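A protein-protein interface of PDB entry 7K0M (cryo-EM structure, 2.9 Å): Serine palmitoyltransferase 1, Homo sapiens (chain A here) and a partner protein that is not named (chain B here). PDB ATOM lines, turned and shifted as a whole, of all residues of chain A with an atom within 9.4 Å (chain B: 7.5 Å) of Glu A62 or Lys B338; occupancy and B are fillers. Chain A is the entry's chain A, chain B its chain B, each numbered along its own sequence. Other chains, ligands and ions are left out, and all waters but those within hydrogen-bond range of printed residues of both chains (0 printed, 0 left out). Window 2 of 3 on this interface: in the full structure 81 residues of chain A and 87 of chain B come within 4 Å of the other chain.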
ATOM      1  N   VAL A  54       9.081 -16.211  20.725  1.00  0.00           N
ATOM      2  CA  VAL A  54      10.282 -15.624  20.132  1.00  0.00           C
ATOM      3  C   VAL A  54      11.328 -16.699  19.860  1.00  0.00           C
ATOM      4  O   VAL A  54      11.941 -16.737  18.786  1.00  0.00           O
ATOM      5  CB  VAL A  54      10.835 -14.511  21.039  1.00  0.00           C
ATOM      6  CG1 VAL A  54      12.228 -14.098  20.591  1.00  0.00           C
ATOM      7  CG2 VAL A  54       9.894 -13.318  21.044  1.00  0.00           C
ATOM      8  N   LYS A  55      11.549 -17.591  20.829  1.00  0.00           N
ATOM      9  CA  LYS A  55      12.509 -18.669  20.619  1.00  0.00           C
ATOM     10  C   LYS A  55      12.048 -19.618  19.519  1.00  0.00           C
ATOM     11  O   LYS A  55      12.876 -20.137  18.761  1.00  0.00           O
ATOM     12  CB  LYS A  55      12.751 -19.427  21.926  1.00  0.00           C
ATOM     13  CG  LYS A  55      11.523 -20.110  22.505  1.00  0.00           C
ATOM     14  CD  LYS A  55      11.841 -20.787  23.825  1.00  0.00           C
ATOM     15  CE  LYS A  55      10.634 -21.534  24.367  1.00  0.00           C
ATOM     16  NZ  LYS A  55       9.528 -20.608  24.736  1.00  0.00           N
ATOM     17  N   GLU A  56      10.738 -19.856  19.415  1.00  0.00           N
ATOM     18  CA  GLU A  56      10.224 -20.685  18.331  1.00  0.00           C
ATOM     19  C   GLU A  56      10.488 -20.044  16.975  1.00  0.00           C
ATOM     20  O   GLU A  56      10.896 -20.723  16.026  1.00  0.00           O
ATOM     21  CB  GLU A  56       8.730 -20.936  18.528  1.00  0.00           C
ATOM     22  CG  GLU A  56       8.403 -21.727  19.782  1.00  0.00           C
ATOM     23  CD  GLU A  56       6.912 -21.881  20.002  1.00  0.00           C
ATOM     24  OE1 GLU A  56       6.132 -21.434  19.136  1.00  0.00           O
ATOM     25  OE2 GLU A  56       6.519 -22.449  21.043  1.00  0.00           O
ATOM     26  N   LYS A  57      10.268 -18.732  16.867  1.00  0.00           N
ATOM     27  CA  LYS A  57      10.572 -18.035  15.623  1.00  0.00           C
ATOM     28  C   LYS A  57      12.057 -18.118  15.300  1.00  0.00           C
ATOM     29  O   LYS A  57      12.437 -18.349  14.146  1.00  0.00           O
ATOM     30  CB  LYS A  57      10.125 -16.578  15.715  1.00  0.00           C
ATOM     31  CG  LYS A  57       8.624 -16.387  15.825  1.00  0.00           C
ATOM     32  CD  LYS A  57       8.283 -14.946  16.160  1.00  0.00           C
ATOM     33  CE  LYS A  57       6.781 -14.731  16.225  1.00  0.00           C
ATOM     34  NZ  LYS A  57       6.118 -15.057  14.934  1.00  0.00           N
ATOM     35  N   GLU A  58      12.913 -17.937  16.308  1.00  0.00           N
ATOM     36  CA  GLU A  58      14.351 -17.980  16.069  1.00  0.00           C
ATOM     37  C   GLU A  58      14.799 -19.361  15.605  1.00  0.00           C
ATOM     38  O   GLU A  58      15.612 -19.479  14.680  1.00  0.00           O
ATOM     39  CB  GLU A  58      15.105 -17.567  17.332  1.00  0.00           C
ATOM     40  CG  GLU A  58      16.616 -17.537  17.169  1.00  0.00           C
ATOM     41  CD  GLU A  58      17.078 -16.480  16.185  1.00  0.00           C
ATOM     42  OE1 GLU A  58      16.357 -15.479  15.998  1.00  0.00           O
ATOM     43  OE2 GLU A  58      18.167 -16.653  15.596  1.00  0.00           O
ATOM     44  N   GLU A  59      14.274 -20.421  16.223  1.00  0.00           N
ATOM     45  CA  GLU A  59      14.667 -21.762  15.801  1.00  0.00           C
ATOM     46  C   GLU A  59      14.105 -22.102  14.425  1.00  0.00           C
ATOM     47  O   GLU A  59      14.779 -22.769  13.630  1.00  0.00           O
ATOM     48  CB  GLU A  59      14.249 -22.796  16.851  1.00  0.00           C
ATOM     49  CG  GLU A  59      12.758 -22.928  17.089  1.00  0.00           C
ATOM     50  CD  GLU A  59      12.118 -24.001  16.235  1.00  0.00           C
ATOM     51  OE1 GLU A  59      12.852 -24.876  15.734  1.00  0.00           O
ATOM     52  OE2 GLU A  59      10.882 -23.969  16.068  1.00  0.00           O
ATOM     53  N   LEU A  60      12.893 -21.632  14.107  1.00  0.00           N
ATOM     54  CA  LEU A  60      12.363 -21.821  12.759  1.00  0.00           C
ATOM     55  C   LEU A  60      13.237 -21.125  11.727  1.00  0.00           C
ATOM     56  O   LEU A  60      13.486 -21.668  10.644  1.00  0.00           O
ATOM     57  CB  LEU A  60      10.928 -21.304  12.673  1.00  0.00           C
ATOM     58  CG  LEU A  60       9.819 -22.180  13.253  1.00  0.00           C
ATOM     59  CD1 LEU A  60       8.506 -21.422  13.274  1.00  0.00           C
ATOM     60  CD2 LEU A  60       9.684 -23.464  12.456  1.00  0.00           C
ATOM     61  N   ILE A  61      13.705 -19.917  12.041  1.00  0.00           N
ATOM     62  CA  ILE A  61      14.625 -19.217  11.152  1.00  0.00           C
ATOM     63  C   ILE A  61      15.917 -20.008  10.999  1.00  0.00           C
ATOM     64  O   ILE A  61      16.475 -20.113   9.900  1.00  0.00           O
ATOM     65  CB  ILE A  61      14.889 -17.793  11.673  1.00  0.00           C
ATOM     66  CG1 ILE A  61      13.631 -16.934  11.540  1.00  0.00           C
ATOM     67  CG2 ILE A  61      16.049 -17.151  10.931  1.00  0.00           C
ATOM     68  CD1 ILE A  61      13.752 -15.579  12.189  1.00  0.00           C
ATOM     69  N   GLU A  62      16.410 -20.584  12.097  1.00  0.00           N
ATOM     70  CA  GLU A  62      17.682 -21.296  12.049  1.00  0.00           C
ATOM     71  C   GLU A  62      17.597 -22.587  11.239  1.00  0.00           C
ATOM     72  O   GLU A  62      18.575 -22.962  10.582  1.00  0.00           O
ATOM     73  CB  GLU A  62      18.175 -21.586  13.466  1.00  0.00           C
ATOM     74  CG  GLU A  62      19.549 -22.229  13.515  1.00  0.00           C
ATOM     75  CD  GLU A  62      20.635 -21.327  12.961  1.00  0.00           C
ATOM     76  OE1 GLU A  62      20.494 -20.091  13.061  1.00  0.00           O
ATOM     77  OE2 GLU A  62      21.628 -21.857  12.421  1.00  0.00           O
ATOM     78  N   GLU A  63      16.458 -23.287  11.273  1.00  0.00           N
ATOM     79  CA  GLU A  63      16.348 -24.523  10.499  1.00  0.00           C
ATOM     80  C   GLU A  63      16.437 -24.265   9.000  1.00  0.00           C
ATOM     81  O   GLU A  63      17.056 -25.046   8.268  1.00  0.00           O
ATOM     82  CB  GLU A  63      15.047 -25.264  10.816  1.00  0.00           C
ATOM     83  CG  GLU A  63      14.746 -25.478  12.282  1.00  0.00           C
ATOM     84  CD  GLU A  63      13.407 -26.156  12.493  1.00  0.00           C
ATOM     85  OE1 GLU A  63      12.607 -26.200  11.535  1.00  0.00           O
ATOM     86  OE2 GLU A  63      13.159 -26.656  13.609  1.00  0.00           O
ATOM     87  N   TRP A  64      15.815 -23.188   8.524  1.00  0.00           N
ATOM     88  CA  TRP A  64      15.676 -22.973   7.087  1.00  0.00           C
ATOM     89  C   TRP A  64      17.035 -22.846   6.410  1.00  0.00           C
ATOM     90  O   TRP A  64      17.929 -22.143   6.890  1.00  0.00           O
ATOM     91  CB  TRP A  64      14.842 -21.721   6.820  1.00  0.00           C
ATOM     92  CG  TRP A  64      14.582 -21.477   5.364  1.00  0.00           C
ATOM     93  CD1 TRP A  64      13.774 -22.206   4.542  1.00  0.00           C
ATOM     94  CD2 TRP A  64      15.136 -20.432   4.557  1.00  0.00           C
ATOM     95  NE1 TRP A  64      13.790 -21.680   3.273  1.00  0.00           N
ATOM     96  CE2 TRP A  64      14.619 -20.590   3.257  1.00  0.00           C
ATOM     97  CE3 TRP A  64      16.018 -19.379   4.808  1.00  0.00           C
ATOM     98  CZ2 TRP A  64      14.955 -19.736   2.214  1.00  0.00           C
ATOM     99  CZ3 TRP A  64      16.349 -18.532   3.772  1.00  0.00           C
ATOM    100  CH2 TRP A  64      15.819 -18.715   2.491  1.00  0.00           C
ATOM    101  N   GLN A  65      17.183 -23.537   5.281  1.00  0.00           N
ATOM    102  CA  GLN A  65      18.409 -23.512   4.491  1.00  0.00           C
ATOM    103  C   GLN A  65      18.026 -23.347   3.027  1.00  0.00           C
ATOM    104  O   GLN A  65      17.322 -24.214   2.472  1.00  0.00           O
ATOM    105  CB  GLN A  65      19.231 -24.785   4.703  1.00  0.00           C
ATOM    106  CG  GLN A  65      20.664 -24.689   4.207  1.00  0.00           C
ATOM    107  CD  GLN A  65      21.467 -23.633   4.940  1.00  0.00           C
ATOM    108  OE1 GLN A  65      21.215 -23.345   6.110  1.00  0.00           O
ATOM    109  NE2 GLN A  65      22.441 -23.051   4.252  1.00  0.00           N
ATOM    110  N   PRO A  66      18.452 -22.277   2.364  1.00  0.00           N
ATOM    111  CA  PRO A  66      18.026 -22.038   0.985  1.00  0.00           C
ATOM    112  C   PRO A  66      18.830 -22.852  -0.018  1.00  0.00           C
ATOM    113  O   PRO A  66      19.923 -23.343   0.263  1.00  0.00           O
ATOM    114  CB  PRO A  66      18.286 -20.542   0.801  1.00  0.00           C
ATOM    115  CG  PRO A  66      19.469 -20.287   1.670  1.00  0.00           C
ATOM    116  CD  PRO A  66      19.328 -21.202   2.863  1.00  0.00           C
ATOM    117  N   GLU A  67      18.256 -22.982  -1.208  1.00  0.00           N
ATOM    118  CA  GLU A  67      18.929 -23.621  -2.323  1.00  0.00           C
ATOM    119  C   GLU A  67      19.993 -22.696  -2.905  1.00  0.00           C
ATOM    120  O   GLU A  67      19.947 -21.480  -2.706  1.00  0.00           O
ATOM    121  CB  GLU A  67      17.917 -23.995  -3.400  1.00  0.00           C
ATOM    122  CG  GLU A  67      16.849 -24.962  -2.936  1.00  0.00           C
ATOM    123  CD  GLU A  67      16.137 -25.627  -4.093  1.00  0.00           C
ATOM    124  OE1 GLU A  67      16.460 -25.303  -5.254  1.00  0.00           O
ATOM    125  OE2 GLU A  67      15.256 -26.476  -3.843  1.00  0.00           O
ATOM    126  N   PRO A  68      20.973 -23.247  -3.618  1.00  0.00           N
ATOM    127  CA  PRO A  68      21.961 -22.391  -4.282  1.00  0.00           C
ATOM    128  C   PRO A  68      21.317 -21.544  -5.368  1.00  0.00           C
ATOM    129  O   PRO A  68      20.288 -21.904  -5.943  1.00  0.00           O
ATOM    130  CB  PRO A  68      22.959 -23.391  -4.874  1.00  0.00           C
ATOM    131  CG  PRO A  68      22.198 -24.663  -4.986  1.00  0.00           C
ATOM    132  CD  PRO A  68      21.274 -24.674  -3.810  1.00  0.00           C
ATOM    133  N   LEU B 292      11.138 -10.303   5.707  1.00  0.00           N
ATOM    134  CA  LEU B 292      12.031 -11.458   5.717  1.00  0.00           C
ATOM    135  C   LEU B 292      11.642 -12.443   6.812  1.00  0.00           C
ATOM    136  O   LEU B 292      11.581 -13.660   6.581  1.00  0.00           O
ATOM    137  CB  LEU B 292      13.476 -10.995   5.892  1.00  0.00           C
ATOM    138  CG  LEU B 292      14.236 -10.664   4.609  1.00  0.00           C
ATOM    139  CD1 LEU B 292      15.521  -9.926   4.926  1.00  0.00           C
ATOM    140  CD2 LEU B 292      14.524 -11.929   3.825  1.00  0.00           C
ATOM    141  N   ILE B 296      10.280 -16.272   6.100  1.00  0.00           N
ATOM    142  CA  ILE B 296      10.984 -17.457   6.584  1.00  0.00           C
ATOM    143  C   ILE B 296      10.097 -18.264   7.525  1.00  0.00           C
ATOM    144  O   ILE B 296      10.098 -19.500   7.491  1.00  0.00           O
ATOM    145  CB  ILE B 296      12.312 -17.063   7.251  1.00  0.00           C
ATOM    146  CG1 ILE B 296      13.244 -16.410   6.234  1.00  0.00           C
ATOM    147  CG2 ILE B 296      12.984 -18.281   7.851  1.00  0.00           C
ATOM    148  CD1 ILE B 296      14.616 -16.102   6.779  1.00  0.00           C
ATOM    149  N   LYS B 309      13.969 -20.112  -2.549  1.00  0.00           N
ATOM    150  CA  LYS B 309      14.970 -19.056  -2.567  1.00  0.00           C
ATOM    151  C   LYS B 309      14.314 -17.748  -2.153  1.00  0.00           C
ATOM    152  O   LYS B 309      13.091 -17.603  -2.204  1.00  0.00           O
ATOM    153  CB  LYS B 309      15.610 -18.905  -3.951  1.00  0.00           C
ATOM    154  CG  LYS B 309      16.829 -19.770  -4.181  1.00  0.00           C
ATOM    155  CD  LYS B 309      17.321 -19.655  -5.610  1.00  0.00           C
ATOM    156  CE  LYS B 309      16.389 -20.362  -6.570  1.00  0.00           C
ATOM    157  NZ  LYS B 309      17.035 -20.589  -7.890  1.00  0.00           N
ATOM    158  N   ILE B 310      15.143 -16.795  -1.734  1.00  0.00           N
ATOM    159  CA  ILE B 310      14.699 -15.438  -1.439  1.00  0.00           C
ATOM    160  C   ILE B 310      15.667 -14.471  -2.106  1.00  0.00           C
ATOM    161  O   ILE B 310      16.871 -14.502  -1.826  1.00  0.00           O
ATOM    162  CB  ILE B 310      14.616 -15.164   0.071  1.00  0.00           C
ATOM    163  CG1 ILE B 310      13.527 -16.025   0.708  1.00  0.00           C
ATOM    164  CG2 ILE B 310      14.342 -13.696   0.326  1.00  0.00           C
ATOM    165  CD1 ILE B 310      13.305 -15.736   2.171  1.00  0.00           C
ATOM    166  N   LEU B 311      15.142 -13.611  -2.973  1.00  0.00           N
ATOM    167  CA  LEU B 311      15.938 -12.653  -3.727  1.00  0.00           C
ATOM    168  C   LEU B 311      15.458 -11.248  -3.400  1.00  0.00           C
ATOM    169  O   LEU B 311      14.251 -10.995  -3.360  1.00  0.00           O
ATOM    170  CB  LEU B 311      15.829 -12.924  -5.229  1.00  0.00           C
ATOM    171  CG  LEU B 311      16.754 -12.161  -6.176  1.00  0.00           C
ATOM    172  CD1 LEU B 311      18.172 -12.687  -6.084  1.00  0.00           C
ATOM    173  CD2 LEU B 311      16.244 -12.259  -7.601  1.00  0.00           C
ATOM    174  N   ILE B 312      16.399 -10.339  -3.164  1.00  0.00           N
ATOM    175  CA  ILE B 312      16.098  -8.951  -2.834  1.00  0.00           C
ATOM    176  C   ILE B 312      16.586  -8.079  -3.978  1.00  0.00           C
ATOM    177  O   ILE B 312      17.792  -8.011  -4.242  1.00  0.00           O
ATOM    178  CB  ILE B 312      16.751  -8.530  -1.509  1.00  0.00           C
ATOM    179  CG1 ILE B 312      16.323  -9.462  -0.379  1.00  0.00           C
ATOM    180  CG2 ILE B 312      16.401  -7.093  -1.177  1.00  0.00           C
ATOM    181  CD1 ILE B 312      17.003  -9.167   0.933  1.00  0.00           C
ATOM    182  N   ALA B 332      23.731  -6.704   5.838  1.00  0.00           N
ATOM    183  CA  ALA B 332      23.629  -7.349   7.143  1.00  0.00           C
ATOM    184  C   ALA B 332      22.364  -8.190   7.250  1.00  0.00           C
ATOM    185  O   ALA B 332      22.399  -9.319   7.752  1.00  0.00           O
ATOM    186  CB  ALA B 332      23.671  -6.299   8.251  1.00  0.00           C
ATOM    187  N   LEU B 333      21.235  -7.657   6.777  1.00  0.00           N
ATOM    188  CA  LEU B 333      19.980  -8.397   6.848  1.00  0.00           C
ATOM    189  C   LEU B 333      20.027  -9.656   5.994  1.00  0.00           C
ATOM    190  O   LEU B 333      19.545 -10.715   6.414  1.00  0.00           O
ATOM    191  CB  LEU B 333      18.819  -7.503   6.417  1.00  0.00           C
ATOM    192  CG  LEU B 333      18.347  -6.485   7.453  1.00  0.00           C
ATOM    193  CD1 LEU B 333      17.274  -5.593   6.870  1.00  0.00           C
ATOM    194  CD2 LEU B 333      17.837  -7.196   8.689  1.00  0.00           C
ATOM    195  N   LYS B 334      20.601  -9.568   4.792  1.00  0.00           N
ATOM    196  CA  LYS B 334      20.655 -10.747   3.938  1.00  0.00           C
ATOM    197  C   LYS B 334      21.627 -11.785   4.482  1.00  0.00           C
ATOM    198  O   LYS B 334      21.406 -12.988   4.303  1.00  0.00           O
ATOM    199  CB  LYS B 334      21.026 -10.361   2.506  1.00  0.00           C
ATOM    200  CG  LYS B 334      22.504 -10.430   2.200  1.00  0.00           C
ATOM    201  CD  LYS B 334      22.766 -10.253   0.729  1.00  0.00           C
ATOM    202  CE  LYS B 334      24.225 -10.486   0.417  1.00  0.00           C
ATOM    203  NZ  LYS B 334      24.591 -11.920   0.559  1.00  0.00           N
ATOM    204  N   LYS B 335      22.704 -11.351   5.141  1.00  0.00           N
ATOM    205  CA  LYS B 335      23.597 -12.310   5.782  1.00  0.00           C
ATOM    206  C   LYS B 335      22.910 -12.992   6.957  1.00  0.00           C
ATOM    207  O   LYS B 335      23.067 -14.201   7.158  1.00  0.00           O
ATOM    208  CB  LYS B 335      24.879 -11.616   6.237  1.00  0.00           C
ATOM    209  CG  LYS B 335      25.812 -11.230   5.106  1.00  0.00           C
ATOM    210  CD  LYS B 335      27.054 -10.537   5.634  1.00  0.00           C
ATOM    211  CE  LYS B 335      28.051 -10.263   4.524  1.00  0.00           C
ATOM    212  NZ  LYS B 335      28.390 -11.496   3.767  1.00  0.00           N
ATOM    213  N   LYS B 336      22.145 -12.233   7.743  1.00  0.00           N
ATOM    214  CA  LYS B 336      21.462 -12.817   8.890  1.00  0.00           C
ATOM    215  C   LYS B 336      20.374 -13.794   8.458  1.00  0.00           C
ATOM    216  O   LYS B 336      20.216 -14.859   9.065  1.00  0.00           O
ATOM    217  CB  LYS B 336      20.874 -11.715   9.768  1.00  0.00           C
ATOM    218  CG  LYS B 336      20.701 -12.115  11.221  1.00  0.00           C
ATOM    219  CD  LYS B 336      20.496 -10.900  12.109  1.00  0.00           C
ATOM    220  CE  LYS B 336      19.022 -10.568  12.262  1.00  0.00           C
ATOM    221  NZ  LYS B 336      18.287 -11.649  12.971  1.00  0.00           N
ATOM    222  N   TYR B 337      19.615 -13.455   7.417  1.00  0.00           N
ATOM    223  CA  TYR B 337      18.460 -14.246   7.015  1.00  0.00           C
ATOM    224  C   TYR B 337      18.725 -15.128   5.802  1.00  0.00           C
ATOM    225  O   TYR B 337      17.794 -15.772   5.308  1.00  0.00           O
ATOM    226  CB  TYR B 337      17.268 -13.330   6.743  1.00  0.00           C
ATOM    227  CG  TYR B 337      16.717 -12.683   7.990  1.00  0.00           C
ATOM    228  CD1 TYR B 337      17.208 -11.467   8.437  1.00  0.00           C
ATOM    229  CD2 TYR B 337      15.711 -13.293   8.724  1.00  0.00           C
ATOM    230  CE1 TYR B 337      16.711 -10.873   9.575  1.00  0.00           C
ATOM    231  CE2 TYR B 337      15.208 -12.705   9.864  1.00  0.00           C
ATOM    232  CZ  TYR B 337      15.711 -11.495  10.286  1.00  0.00           C
ATOM    233  OH  TYR B 337      15.216 -10.902  11.423  1.00  0.00           O
ATOM    234  N   LYS B 338      19.965 -15.172   5.312  1.00  0.00           N
ATOM    235  CA  LYS B 338      20.361 -16.046   4.207  1.00  0.00           C
ATOM    236  C   LYS B 338      19.520 -15.784   2.956  1.00  0.00           C
ATOM    237  O   LYS B 338      18.784 -16.646   2.473  1.00  0.00           O
ATOM    238  CB  LYS B 338      20.288 -17.520   4.624  1.00  0.00           C
ATOM    239  CG  LYS B 338      21.251 -17.900   5.736  1.00  0.00           C
ATOM    240  CD  LYS B 338      20.867 -19.225   6.373  1.00  0.00           C
ATOM    241  CE  LYS B 338      19.546 -19.122   7.114  1.00  0.00           C
ATOM    242  NZ  LYS B 338      19.217 -20.382   7.832  1.00  0.00           N
ATOM    243  N   ALA B 339      19.644 -14.568   2.436  1.00  0.00           N
ATOM    244  CA  ALA B 339      18.971 -14.157   1.213  1.00  0.00           C
ATOM    245  C   ALA B 339      20.006 -13.752   0.172  1.00  0.00           C
ATOM    246  O   ALA B 339      21.176 -13.515   0.483  1.00  0.00           O
ATOM    247  CB  ALA B 339      17.997 -13.004   1.478  1.00  0.00           C
ATOM    248  N   TYR B 340      19.566 -13.676  -1.079  1.00  0.00           N
ATOM    249  CA  TYR B 340      20.424 -13.294  -2.189  1.00  0.00           C
ATOM    250  C   TYR B 340      20.124 -11.859  -2.601  1.00  0.00           C
ATOM    251  O   TYR B 340      19.001 -11.376  -2.442  1.00  0.00           O
ATOM    252  CB  TYR B 340      20.232 -14.237  -3.377  1.00  0.00           C
ATOM    253  CG  TYR B 340      20.511 -15.683  -3.048  1.00  0.00           C
ATOM    254  CD1 TYR B 340      21.768 -16.088  -2.627  1.00  0.00           C
ATOM    255  CD2 TYR B 340      19.517 -16.644  -3.153  1.00  0.00           C
ATOM    256  CE1 TYR B 340      22.028 -17.406  -2.323  1.00  0.00           C
ATOM    257  CE2 TYR B 340      19.768 -17.964  -2.852  1.00  0.00           C
ATOM    258  CZ  TYR B 340      21.025 -18.339  -2.437  1.00  0.00           C
ATOM    259  OH  TYR B 340      21.280 -19.655  -2.135  1.00  0.00           O
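Among the printed residues, pairs that only touch across the chains: Trp A64 with Tyr B337 (3.5 Å), Pro A68 with Tyr B340 (3.5 Å), Pro A68 with Lys B309 (3.7 Å), Pro A66 with Lys B338 (3.8 Å), Ile A61 with Ile B296 (3.8 Å), Glu A62 with Lys B338 (3.8 Å), Glu A67 with Lys B309 (3.8 Å), Trp A64 with Ile B310 (3.9 Å), Gln A65 with Lys B338 (3.97 Å) and Ile A61 with Tyr B337 (3.97 Å).
The backbone carbonyl oxygen (O) of Ile B310 sits at hydrogen-bond distance from the backbone NH (N) of Tyr B340, at 2.9 Å.
The backbone NH (N) of Ile B312 lies within hydrogen-bond range of the backbone carbonyl oxygen (O) of Tyr B340 (2.9 Å).
O of Ile A61 is in hydrogen-bond range of NZ of Lys B338, 3.4 Å away.
The backbone carbonyl oxygen (O) of Trp A64 sits close to the side-chain amino group (NZ) of Lys B338.
O of Glu A67 sits close to OH of Tyr B340 (2.3 Å).
Glu A62 touches just one residue of chain B: Lys B338 (3.8 Å).
Of chain A, only Ile A61, Glu A62, Trp A64, Gln A65 and Pro A66 come within 4 Å of Lys B338.
Of the printed residues of chain A, Lys B309 touches Glu A67 and Pro A68.
Of the printed residues of chain B, Gln A65 touches Lys B338.
Printed residues of chain B within 4 Å of Pro A68: Lys B309 and Tyr B340.
Of the printed residues of chain A, Ile B296 touches Ile A61 (3.8 Å).
The nearest residue of chain A that does not touch Lys B338 is Glu A63 (4.9 Å).
The nearest printed residue of chain B that does not touch Gln A65 is Tyr B340 (7.1 Å).
Of the 15 printed residues of chain B, 6 touch a printed residue of chain A.
Hydrophobic or aromatic side chains of chain B within 4 Å of the printed part of chain A: Ile B296, Ile B310, Tyr B337 and Tyr B340.
Printed residues of chain A that touch a printed residue of chain B: Ile A61, Glu A62, Trp A64, Gln A65, Pro A66, Glu A67 and Pro A68.
Among the printed residues, no Asp or Glu carboxylate lies within 4 Å of a Lys or Arg side-chain nitrogen of the other chain.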
